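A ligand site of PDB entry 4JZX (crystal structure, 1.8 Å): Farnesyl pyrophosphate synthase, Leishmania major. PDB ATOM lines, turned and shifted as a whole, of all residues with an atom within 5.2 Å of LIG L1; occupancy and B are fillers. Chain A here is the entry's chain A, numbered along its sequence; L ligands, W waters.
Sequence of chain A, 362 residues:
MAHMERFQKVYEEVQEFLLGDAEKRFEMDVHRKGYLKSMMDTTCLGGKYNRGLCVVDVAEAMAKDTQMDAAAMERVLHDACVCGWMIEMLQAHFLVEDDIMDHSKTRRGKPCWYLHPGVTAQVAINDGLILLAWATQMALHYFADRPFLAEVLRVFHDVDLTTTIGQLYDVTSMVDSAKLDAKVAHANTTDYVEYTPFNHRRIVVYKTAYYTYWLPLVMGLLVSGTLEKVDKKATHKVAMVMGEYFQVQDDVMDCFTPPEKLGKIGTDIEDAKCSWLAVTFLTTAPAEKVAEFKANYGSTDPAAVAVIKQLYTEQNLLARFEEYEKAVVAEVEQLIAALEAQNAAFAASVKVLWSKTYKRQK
Merely in contact with LIG L1: Gly 47 (3.3 Å), Leu 95 (3.96 Å), Thr 208 (3.5 Å), Tyr 211 (3.3 Å), Phe 246 (3.6 Å), Gln 247 (3.5 Å) and Asp 250 (3.4 Å).
Hydrophobic or aromatic side chains within 4 Å of LIG L1: Leu 95 and Phe 246.
11 residues have an atom within 4 Å of LIG L1: Gly 47, Lys 48, Arg 51, Gln 91, Leu 95, Arg 108, Thr 208, Tyr 211, Phe 246, Gln 247 and Asp 250.
The guanidinium group of Arg 107 lies within salt-bridge range of an oxygen (O1) of LG2 L2 (2.8 Å).
NE of Arg 108 lies within salt-bridge range of O7 of LIG L1.
An oxygen (O1) of LG2 L2 is in salt-bridge range of the side-chain amino group (NZ) of Lys 264, at 2.9 Å.
N of Lys 48 sits at hydrogen-bond distance from O5 of LIG L1.
An oxygen (O3) of LIG L1 is in salt-bridge range of the side-chain amino group of Lys 48 (2.7 Å).
The side-chain amide oxygen (OE1) of Gln 91 lies close to an oxygen (O6) of LIG L1 (2.9 Å).
NH1 of Arg 51 lies within salt-bridge range of O2 of LIG L1, 2.8 Å away.
Water W5 lies within hydrogen-bond range of O7 of LIG L1 (2.7 Å) and NH1 of Arg 107 (3.0 Å).
Water W2 lies within hydrogen-bond range of NZ of Lys 264 and O3 of LIG L1.
Water W6 lies within hydrogen-bond range of an oxygen (O6) of LIG L1 (2.7 Å), the side-chain carboxylate of Glu 88 (2.8 Å), the backbone NH of Tyr 49 (3.1 Å) and the backbone NH of Lys 48 (3.4 Å).
Water W1 lies within hydrogen-bond range of O5 of LIG L1, N of Tyr 49 and NH1 of Arg 51.
Water W4 lies within hydrogen-bond range of OD1 of Asp 250 (2.8 Å), NH1 of Arg 360 (2.8 Å) and O3 of LIG L1 (2.9 Å).
Water W3 bridges O7 of LIG L1 (2.9 Å) and NZ of Lys 48 (3.1 Å).
O of Thr 208 is in hydrogen-bond range of OG1 of Thr 212 (2.9 Å).
O of Phe 246 is in hydrogen-bond range of NH2 of Arg 360 (3.0 Å).
The side-chain hydroxyl (OH) of Tyr 211 is in hydrogen-bond range of the side-chain amide nitrogen (NE2) of Gln 91 (2.7 Å).
OH of Tyr 211 lies within hydrogen-bond range of NH2 of Arg 51 (3.4 Å).
NH1 of Arg 51 is in hydrogen-bond range of OE1 of Gln 91 (3.2 Å).
The side-chain hydroxyl of Thr 208 lies within hydrogen-bond range of the side-chain amide oxygen of Gln 247 (2.7 Å).
The guanidinium group (NH2) of Arg 51 is in hydrogen-bond range of the side-chain hydroxyl (OG1) of Thr 212 (3.0 Å).
NZ of Lys 264 lies within salt-bridge range of OD1 of Asp 250 (2.8 Å).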
ATOM      1  N   GLY A  46      -4.317 -13.498   7.650  1.00  0.00           N
ATOM      2  CA  GLY A  46      -4.653 -14.859   8.034  1.00  0.00           C
ATOM      3  C   GLY A  46      -6.135 -15.221   8.000  1.00  0.00           C
ATOM      4  O   GLY A  46      -6.482 -16.388   8.147  1.00  0.00           O
ATOM      5  N   GLY A  47      -6.988 -14.225   7.825  1.00  0.00           N
ATOM      6  CA  GLY A  47      -8.433 -14.452   7.692  1.00  0.00           C
ATOM      7  C   GLY A  47      -8.786 -14.801   6.255  1.00  0.00           C
ATOM      8  O   GLY A  47      -7.890 -15.010   5.430  1.00  0.00           O
ATOM      9  N   LYS A  48     -10.087 -14.868   5.959  1.00  0.00           N
ATOM     10  CA  LYS A  48     -10.541 -15.259   4.610  1.00  0.00           C
ATOM     11  C   LYS A  48     -10.576 -14.082   3.625  1.00  0.00           C
ATOM     12  O   LYS A  48     -10.641 -14.276   2.404  1.00  0.00           O
ATOM     13  CB  LYS A  48     -11.918 -15.933   4.686  1.00  0.00           C
ATOM     14  CG  LYS A  48     -12.009 -17.107   5.658  1.00  0.00           C
ATOM     15  CD  LYS A  48     -13.451 -17.598   5.825  1.00  0.00           C
ATOM     16  CE  LYS A  48     -14.219 -16.791   6.868  1.00  0.00           C
ATOM     17  NZ  LYS A  48     -13.778 -17.185   8.249  1.00  0.00           N
ATOM     18  N   TYR A  49     -10.516 -12.874   4.181  1.00  0.00           N
ATOM     19  CA  TYR A  49     -10.631 -11.608   3.413  1.00  0.00           C
ATOM     20  C   TYR A  49     -11.955 -11.412   2.676  1.00  0.00           C
ATOM     21  O   TYR A  49     -12.013 -10.641   1.706  1.00  0.00           O
ATOM     22  CB  TYR A  49      -9.436 -11.404   2.456  1.00  0.00           C
ATOM     23  CG  TYR A  49      -8.085 -11.698   3.078  1.00  0.00           C
ATOM     24  CD1 TYR A  49      -7.402 -12.882   2.786  1.00  0.00           C
ATOM     25  CD2 TYR A  49      -7.487 -10.795   3.969  1.00  0.00           C
ATOM     26  CE1 TYR A  49      -6.142 -13.159   3.356  1.00  0.00           C
ATOM     27  CE2 TYR A  49      -6.249 -11.062   4.540  1.00  0.00           C
ATOM     28  CZ  TYR A  49      -5.583 -12.243   4.243  1.00  0.00           C
ATOM     29  OH  TYR A  49      -4.352 -12.505   4.820  1.00  0.00           O
ATOM     30  N   ARG A  51     -14.549  -9.747   3.479  1.00  0.00           N
ATOM     31  CA  ARG A  51     -15.000  -8.340   3.540  1.00  0.00           C
ATOM     32  C   ARG A  51     -14.216  -7.460   2.572  1.00  0.00           C
ATOM     33  O   ARG A  51     -14.809  -6.748   1.766  1.00  0.00           O
ATOM     34  CB  ARG A  51     -14.889  -7.779   4.958  1.00  0.00           C
ATOM     35  CG  ARG A  51     -15.816  -8.446   5.972  1.00  0.00           C
ATOM     36  CD  ARG A  51     -15.391  -8.070   7.384  1.00  0.00           C
ATOM     37  NE  ARG A  51     -16.132  -8.843   8.388  1.00  0.00           N
ATOM     38  CZ  ARG A  51     -15.819 -10.092   8.752  1.00  0.00           C
ATOM     39  NH1 ARG A  51     -14.789 -10.723   8.190  1.00  0.00           N
ATOM     40  NH2 ARG A  51     -16.536 -10.710   9.677  1.00  0.00           N
ATOM     41  N   GLU A  88     -10.944  -4.645   6.667  1.00  0.00           N
ATOM     42  CA  GLU A  88     -10.105  -5.685   7.275  1.00  0.00           C
ATOM     43  C   GLU A  88      -9.439  -5.217   8.571  1.00  0.00           C
ATOM     44  O   GLU A  88      -9.272  -5.996   9.502  1.00  0.00           O
ATOM     45  CB  GLU A  88      -9.059  -6.213   6.288  1.00  0.00           C
ATOM     46  CG  GLU A  88      -9.660  -7.015   5.108  1.00  0.00           C
ATOM     47  CD  GLU A  88     -10.409  -8.270   5.528  1.00  0.00           C
ATOM     48  OE1 GLU A  88     -10.070  -8.869   6.570  1.00  0.00           O
ATOM     49  OE2 GLU A  88     -11.319  -8.685   4.788  1.00  0.00           O
ATOM     50  N   GLN A  91     -12.180  -5.091  11.194  1.00  0.00           N
ATOM     51  CA  GLN A  91     -12.248  -6.489  11.626  1.00  0.00           C
ATOM     52  C   GLN A  91     -11.110  -6.792  12.610  1.00  0.00           C
ATOM     53  O   GLN A  91     -11.367  -7.346  13.680  1.00  0.00           O
ATOM     54  CB  GLN A  91     -12.181  -7.420  10.396  1.00  0.00           C
ATOM     55  CG  GLN A  91     -11.884  -8.905  10.702  1.00  0.00           C
ATOM     56  CD  GLN A  91     -13.080  -9.669  11.249  1.00  0.00           C
ATOM     57  OE1 GLN A  91     -13.252 -10.871  10.956  1.00  0.00           O
ATOM     58  NE2 GLN A  91     -13.905  -9.004  12.044  1.00  0.00           N
ATOM     59  N   LEU A  95     -11.625  -8.042  16.470  1.00  0.00           N
ATOM     60  CA  LEU A  95     -11.182  -9.350  16.946  1.00  0.00           C
ATOM     61  C   LEU A  95     -10.162  -9.254  18.083  1.00  0.00           C
ATOM     62  O   LEU A  95     -10.229 -10.049  19.029  1.00  0.00           O
ATOM     63  CB  LEU A  95     -10.661 -10.230  15.809  1.00  0.00           C
ATOM     64  CG  LEU A  95     -11.594 -10.504  14.619  1.00  0.00           C
ATOM     65  CD1 LEU A  95     -10.972 -11.546  13.677  1.00  0.00           C
ATOM     66  CD2 LEU A  95     -12.985 -10.926  15.068  1.00  0.00           C
ATOM     67  N   ARG A 107      -6.786 -17.523  17.528  1.00  0.00           N
ATOM     68  CA  ARG A 107      -7.393 -16.765  16.444  1.00  0.00           C
ATOM     69  C   ARG A 107      -6.638 -17.046  15.162  1.00  0.00           C
ATOM     70  O   ARG A 107      -5.424 -16.890  15.131  1.00  0.00           O
ATOM     71  CB  ARG A 107      -7.334 -15.256  16.745  1.00  0.00           C
ATOM     72  CG  ARG A 107      -7.833 -14.363  15.595  1.00  0.00           C
ATOM     73  CD  ARG A 107      -9.320 -14.571  15.330  1.00  0.00           C
ATOM     74  NE  ARG A 107     -10.176 -14.082  16.416  1.00  0.00           N
ATOM     75  CZ  ARG A 107     -11.501 -14.159  16.411  1.00  0.00           C
ATOM     76  NH1 ARG A 107     -12.138 -14.699  15.380  1.00  0.00           N
ATOM     77  NH2 ARG A 107     -12.211 -13.695  17.446  1.00  0.00           N
ATOM     78  N   ARG A 108      -7.364 -17.466  14.123  1.00  0.00           N
ATOM     79  CA  ARG A 108      -6.784 -17.751  12.796  1.00  0.00           C
ATOM     80  C   ARG A 108      -5.579 -18.705  12.900  1.00  0.00           C
ATOM     81  O   ARG A 108      -4.560 -18.529  12.225  1.00  0.00           O
ATOM     82  CB  ARG A 108      -6.414 -16.448  12.048  1.00  0.00           C
ATOM     83  CG  ARG A 108      -7.613 -15.551  11.734  1.00  0.00           C
ATOM     84  CD  ARG A 108      -7.160 -14.165  11.296  1.00  0.00           C
ATOM     85  NE  ARG A 108      -8.274 -13.300  10.919  1.00  0.00           N
ATOM     86  CZ  ARG A 108      -8.187 -11.981  10.760  1.00  0.00           C
ATOM     87  NH1 ARG A 108      -7.026 -11.354  10.936  1.00  0.00           N
ATOM     88  NH2 ARG A 108      -9.260 -11.281  10.406  1.00  0.00           N
ATOM     89  N   THR A 208     -22.717  -8.179  13.607  1.00  0.00           N
ATOM     90  CA  THR A 208     -22.078  -8.858  12.468  1.00  0.00           C
ATOM     91  C   THR A 208     -22.522  -8.393  11.080  1.00  0.00           C
ATOM     92  O   THR A 208     -21.676  -8.093  10.225  1.00  0.00           O
ATOM     93  CB  THR A 208     -22.228 -10.403  12.591  1.00  0.00           C
ATOM     94  OG1 THR A 208     -21.453 -10.869  13.694  1.00  0.00           O
ATOM     95  CG2 THR A 208     -21.765 -11.135  11.287  1.00  0.00           C
ATOM     96  N   TYR A 211     -21.205  -4.779   9.502  1.00  0.00           N
ATOM     97  CA  TYR A 211     -19.807  -4.634   9.089  1.00  0.00           C
ATOM     98  C   TYR A 211     -19.321  -5.734   8.153  1.00  0.00           C
ATOM     99  O   TYR A 211     -18.346  -5.539   7.413  1.00  0.00           O
ATOM    100  CB  TYR A 211     -18.874  -4.460  10.289  1.00  0.00           C
ATOM    101  CG  TYR A 211     -18.257  -5.706  10.885  1.00  0.00           C
ATOM    102  CD1 TYR A 211     -16.945  -6.081  10.572  1.00  0.00           C
ATOM    103  CD2 TYR A 211     -18.960  -6.469  11.820  1.00  0.00           C
ATOM    104  CE1 TYR A 211     -16.363  -7.211  11.141  1.00  0.00           C
ATOM    105  CE2 TYR A 211     -18.383  -7.601  12.402  1.00  0.00           C
ATOM    106  CZ  TYR A 211     -17.092  -7.970  12.060  1.00  0.00           C
ATOM    107  OH  TYR A 211     -16.544  -9.078  12.658  1.00  0.00           O
ATOM    108  N   THR A 212     -20.004  -6.869   8.160  1.00  0.00           N
ATOM    109  CA  THR A 212     -19.571  -8.003   7.345  1.00  0.00           C
ATOM    110  C   THR A 212     -20.242  -8.050   5.972  1.00  0.00           C
ATOM    111  O   THR A 212     -19.635  -8.515   5.008  1.00  0.00           O
ATOM    112  CB  THR A 212     -19.724  -9.346   8.102  1.00  0.00           C
ATOM    113  OG1 THR A 212     -19.105  -9.234   9.397  1.00  0.00           O
ATOM    114  CG2 THR A 212     -19.064 -10.487   7.334  1.00  0.00           C
ATOM    115  N   PHE A 246     -24.806 -15.732   8.138  1.00  0.00           N
ATOM    116  CA  PHE A 246     -23.352 -15.842   8.389  1.00  0.00           C
ATOM    117  C   PHE A 246     -23.055 -16.052   9.872  1.00  0.00           C
ATOM    118  O   PHE A 246     -22.270 -16.925  10.234  1.00  0.00           O
ATOM    119  CB  PHE A 246     -22.618 -14.612   7.832  1.00  0.00           C
ATOM    120  CG  PHE A 246     -21.123 -14.630   8.093  1.00  0.00           C
ATOM    121  CD1 PHE A 246     -20.603 -14.063   9.262  1.00  0.00           C
ATOM    122  CD2 PHE A 246     -20.247 -15.207   7.169  1.00  0.00           C
ATOM    123  CE1 PHE A 246     -19.209 -14.057   9.507  1.00  0.00           C
ATOM    124  CE2 PHE A 246     -18.860 -15.193   7.383  1.00  0.00           C
ATOM    125  CZ  PHE A 246     -18.342 -14.634   8.572  1.00  0.00           C
ATOM    126  N   GLN A 247     -23.679 -15.254  10.744  1.00  0.00           N
ATOM    127  CA  GLN A 247     -23.462 -15.406  12.193  1.00  0.00           C
ATOM    128  C   GLN A 247     -24.071 -16.687  12.764  1.00  0.00           C
ATOM    129  O   GLN A 247     -23.508 -17.296  13.678  1.00  0.00           O
ATOM    130  CB  GLN A 247     -23.978 -14.191  12.967  1.00  0.00           C
ATOM    131  CG  GLN A 247     -23.505 -14.185  14.417  1.00  0.00           C
ATOM    132  CD  GLN A 247     -21.994 -14.295  14.544  1.00  0.00           C
ATOM    133  OE1 GLN A 247     -21.252 -13.532  13.931  1.00  0.00           O
ATOM    134  NE2 GLN A 247     -21.530 -15.255  15.343  1.00  0.00           N
ATOM    135  N   ASP A 250     -21.570 -19.270  12.053  1.00  0.00           N
ATOM    136  CA  ASP A 250     -20.516 -19.104  13.038  1.00  0.00           C
ATOM    137  C   ASP A 250     -20.894 -19.724  14.381  1.00  0.00           C
ATOM    138  O   ASP A 250     -20.091 -20.431  14.996  1.00  0.00           O
ATOM    139  CB  ASP A 250     -20.147 -17.621  13.185  1.00  0.00           C
ATOM    140  CG  ASP A 250     -18.939 -17.410  14.055  1.00  0.00           C
ATOM    141  OD1 ASP A 250     -17.815 -17.688  13.584  1.00  0.00           O
ATOM    142  OD2 ASP A 250     -19.107 -16.975  15.211  1.00  0.00           O
ATOM    143  N   LYS A 264     -10.025 -21.281  15.546  1.00  0.00           N
ATOM    144  CA  LYS A 264     -10.304 -20.649  16.832  1.00  0.00           C
ATOM    145  C   LYS A 264     -11.018 -21.627  17.751  1.00  0.00           C
ATOM    146  O   LYS A 264     -11.618 -22.595  17.273  1.00  0.00           O
ATOM    147  CB  LYS A 264     -11.145 -19.366  16.653  1.00  0.00           C
ATOM    148  CG  LYS A 264     -12.543 -19.595  16.077  1.00  0.00           C
ATOM    149  CD  LYS A 264     -13.172 -18.311  15.556  1.00  0.00           C
ATOM    150  CE  LYS A 264     -14.568 -18.593  14.990  1.00  0.00           C
ATOM    151  NZ  LYS A 264     -15.149 -17.384  14.326  1.00  0.00           N
ATOM    152  N   ARG A 360     -20.359 -22.473   3.604  1.00  0.00           N
ATOM    153  CA  ARG A 360     -18.937 -22.361   3.954  1.00  0.00           C
ATOM    154  C   ARG A 360     -18.618 -23.332   5.093  1.00  0.00           C
ATOM    155  O   ARG A 360     -19.507 -23.733   5.837  1.00  0.00           O
ATOM    156  CB  ARG A 360     -18.550 -20.919   4.329  1.00  0.00           C
ATOM    157  CG  ARG A 360     -19.065 -20.461   5.700  1.00  0.00           C
ATOM    158  CD  ARG A 360     -18.949 -18.952   5.878  1.00  0.00           C
ATOM    159  NE  ARG A 360     -19.566 -18.507   7.122  1.00  0.00           N
ATOM    160  CZ  ARG A 360     -18.912 -18.279   8.264  1.00  0.00           C
ATOM    161  NH1 ARG A 360     -17.583 -18.435   8.353  1.00  0.00           N
ATOM    162  NH2 ARG A 360     -19.590 -17.848   9.328  1.00  0.00           N
ATOM    163  N   LYS A 362     -15.647 -22.864   7.119  1.00  0.00           N
ATOM    164  CA  LYS A 362     -14.863 -22.124   8.113  1.00  0.00           C
ATOM    165  C   LYS A 362     -15.048 -20.612   7.916  1.00  0.00           C
ATOM    166  O   LYS A 362     -14.526 -19.826   8.706  1.00  0.00           O
ATOM    167  CB  LYS A 362     -13.378 -22.493   8.034  1.00  0.00           C
ATOM    168  CG  LYS A 362     -12.667 -22.038   6.761  1.00  0.00           C
ATOM    169  CD  LYS A 362     -11.149 -22.131   6.901  1.00  0.00           C
ATOM    170  CE  LYS A 362     -10.566 -20.850   7.510  1.00  0.00           C
ATOM    171  NZ  LYS A 362      -9.069 -20.922   7.593  1.00  0.00           N
ATOM    172  OXT LYS A 362     -15.704 -20.169   6.972  1.00  0.00           O
HETATM  173  C1  LIG L   1     -15.044 -13.594  12.521  1.00  0.00           C
HETATM  174  O1  LIG L   1     -15.255 -13.295  11.139  1.00  0.00           O
HETATM  175  C2  LIG L   1     -16.034 -12.797  13.381  1.00  0.00           C
HETATM  176  C3  LIG L   1     -17.467 -13.057  12.977  1.00  0.00           C
HETATM  177  C4  LIG L   1     -18.002 -14.278  13.017  1.00  0.00           C
HETATM  178  C5  LIG L   1     -18.296 -11.905  12.500  1.00  0.00           C
HETATM  179  P1  LIG L   1     -14.603 -14.174   9.964  1.00  0.00           P
HETATM  180  O2  LIG L   1     -14.928 -13.482   8.675  1.00  0.00           O
HETATM  181  O3  LIG L   1     -15.036 -15.626  10.114  1.00  0.00           O
HETATM  182  O4  LIG L   1     -13.015 -14.105  10.284  1.00  0.00           O
HETATM  183  P2  LIG L   1     -11.723 -13.916   9.297  1.00  0.00           P
HETATM  184  O5  LIG L   1     -12.002 -14.593   7.980  1.00  0.00           O
HETATM  185  O6  LIG L   1     -11.541 -12.416   9.195  1.00  0.00           O
HETATM  186  O7  LIG L   1     -10.663 -14.573  10.158  1.00  0.00           O
HETATM  187  O1  LG2 L   2     -14.913 -14.860  15.748  1.00  0.00           O
HETATM  188  P1  LG2 L   2     -15.622 -15.091  17.072  1.00  0.00           P
HETATM  189  O2  LG2 L   2     -14.754 -14.761  18.262  1.00  0.00           O
HETATM  190  O3  LG2 L   2     -16.285 -16.441  17.149  1.00  0.00           O
HETATM  191  C1  LG2 L   2     -16.958 -13.823  17.068  1.00  0.00           C
HETATM  192  P2  LG2 L   2     -18.137 -13.916  18.458  1.00  0.00           P
HETATM  193  O4  LG2 L   2     -17.365 -13.852  19.762  1.00  0.00           O
HETATM  194  O5  LG2 L   2     -19.098 -12.770  18.281  1.00  0.00           O
HETATM  195  O6  LG2 L   2     -18.858 -15.244  18.277  1.00  0.00           O
HETATM  196  C2  LG2 L   2     -16.228 -12.472  16.999  1.00  0.00           C
HETATM  197  N1  LG2 L   2     -17.039 -11.264  16.775  1.00  0.00           N
HETATM  198  C3  LG2 L   2     -16.638 -10.172  17.441  1.00  0.00           C
HETATM  199  C4  LG2 L   2     -17.297  -8.956  17.339  1.00  0.00           C
HETATM  200  C5  LG2 L   2     -18.396  -8.870  16.483  1.00  0.00           C
HETATM  201  C6  LG2 L   2     -18.805 -10.012  15.778  1.00  0.00           C
HETATM  202  C7  LG2 L   2     -18.095 -11.214  15.930  1.00  0.00           C
HETATM  203  C8  LG2 L   2     -16.732  -7.820  18.180  1.00  0.00           C
HETATM  204  C9  LG2 L   2     -17.301  -6.430  17.942  1.00  0.00           C
HETATM  205  C10 LG2 L   2     -16.712  -5.476  18.971  1.00  0.00           C
HETATM  206  C11 LG2 L   2     -17.341  -4.095  18.877  1.00  0.00           C
HETATM  207  O   HOH W   1     -13.323 -13.074   6.100  1.00  0.00           O
HETATM  208  O   HOH W   2     -13.742 -17.069  12.025  1.00  0.00           O
HETATM  209  O   HOH W   3     -10.875 -17.309   9.258  1.00  0.00           O
HETATM  210  O   HOH W   4     -17.169 -17.390  10.923  1.00  0.00           O
HETATM  211  O   HOH W   5     -11.361 -15.586  12.576  1.00  0.00           O
HETATM  212  O   HOH W   6     -10.228 -11.597   6.940  1.00  0.00           O
HETATM  213  O   HOH W   7     -16.071 -13.631   6.292  1.00  0.00           O
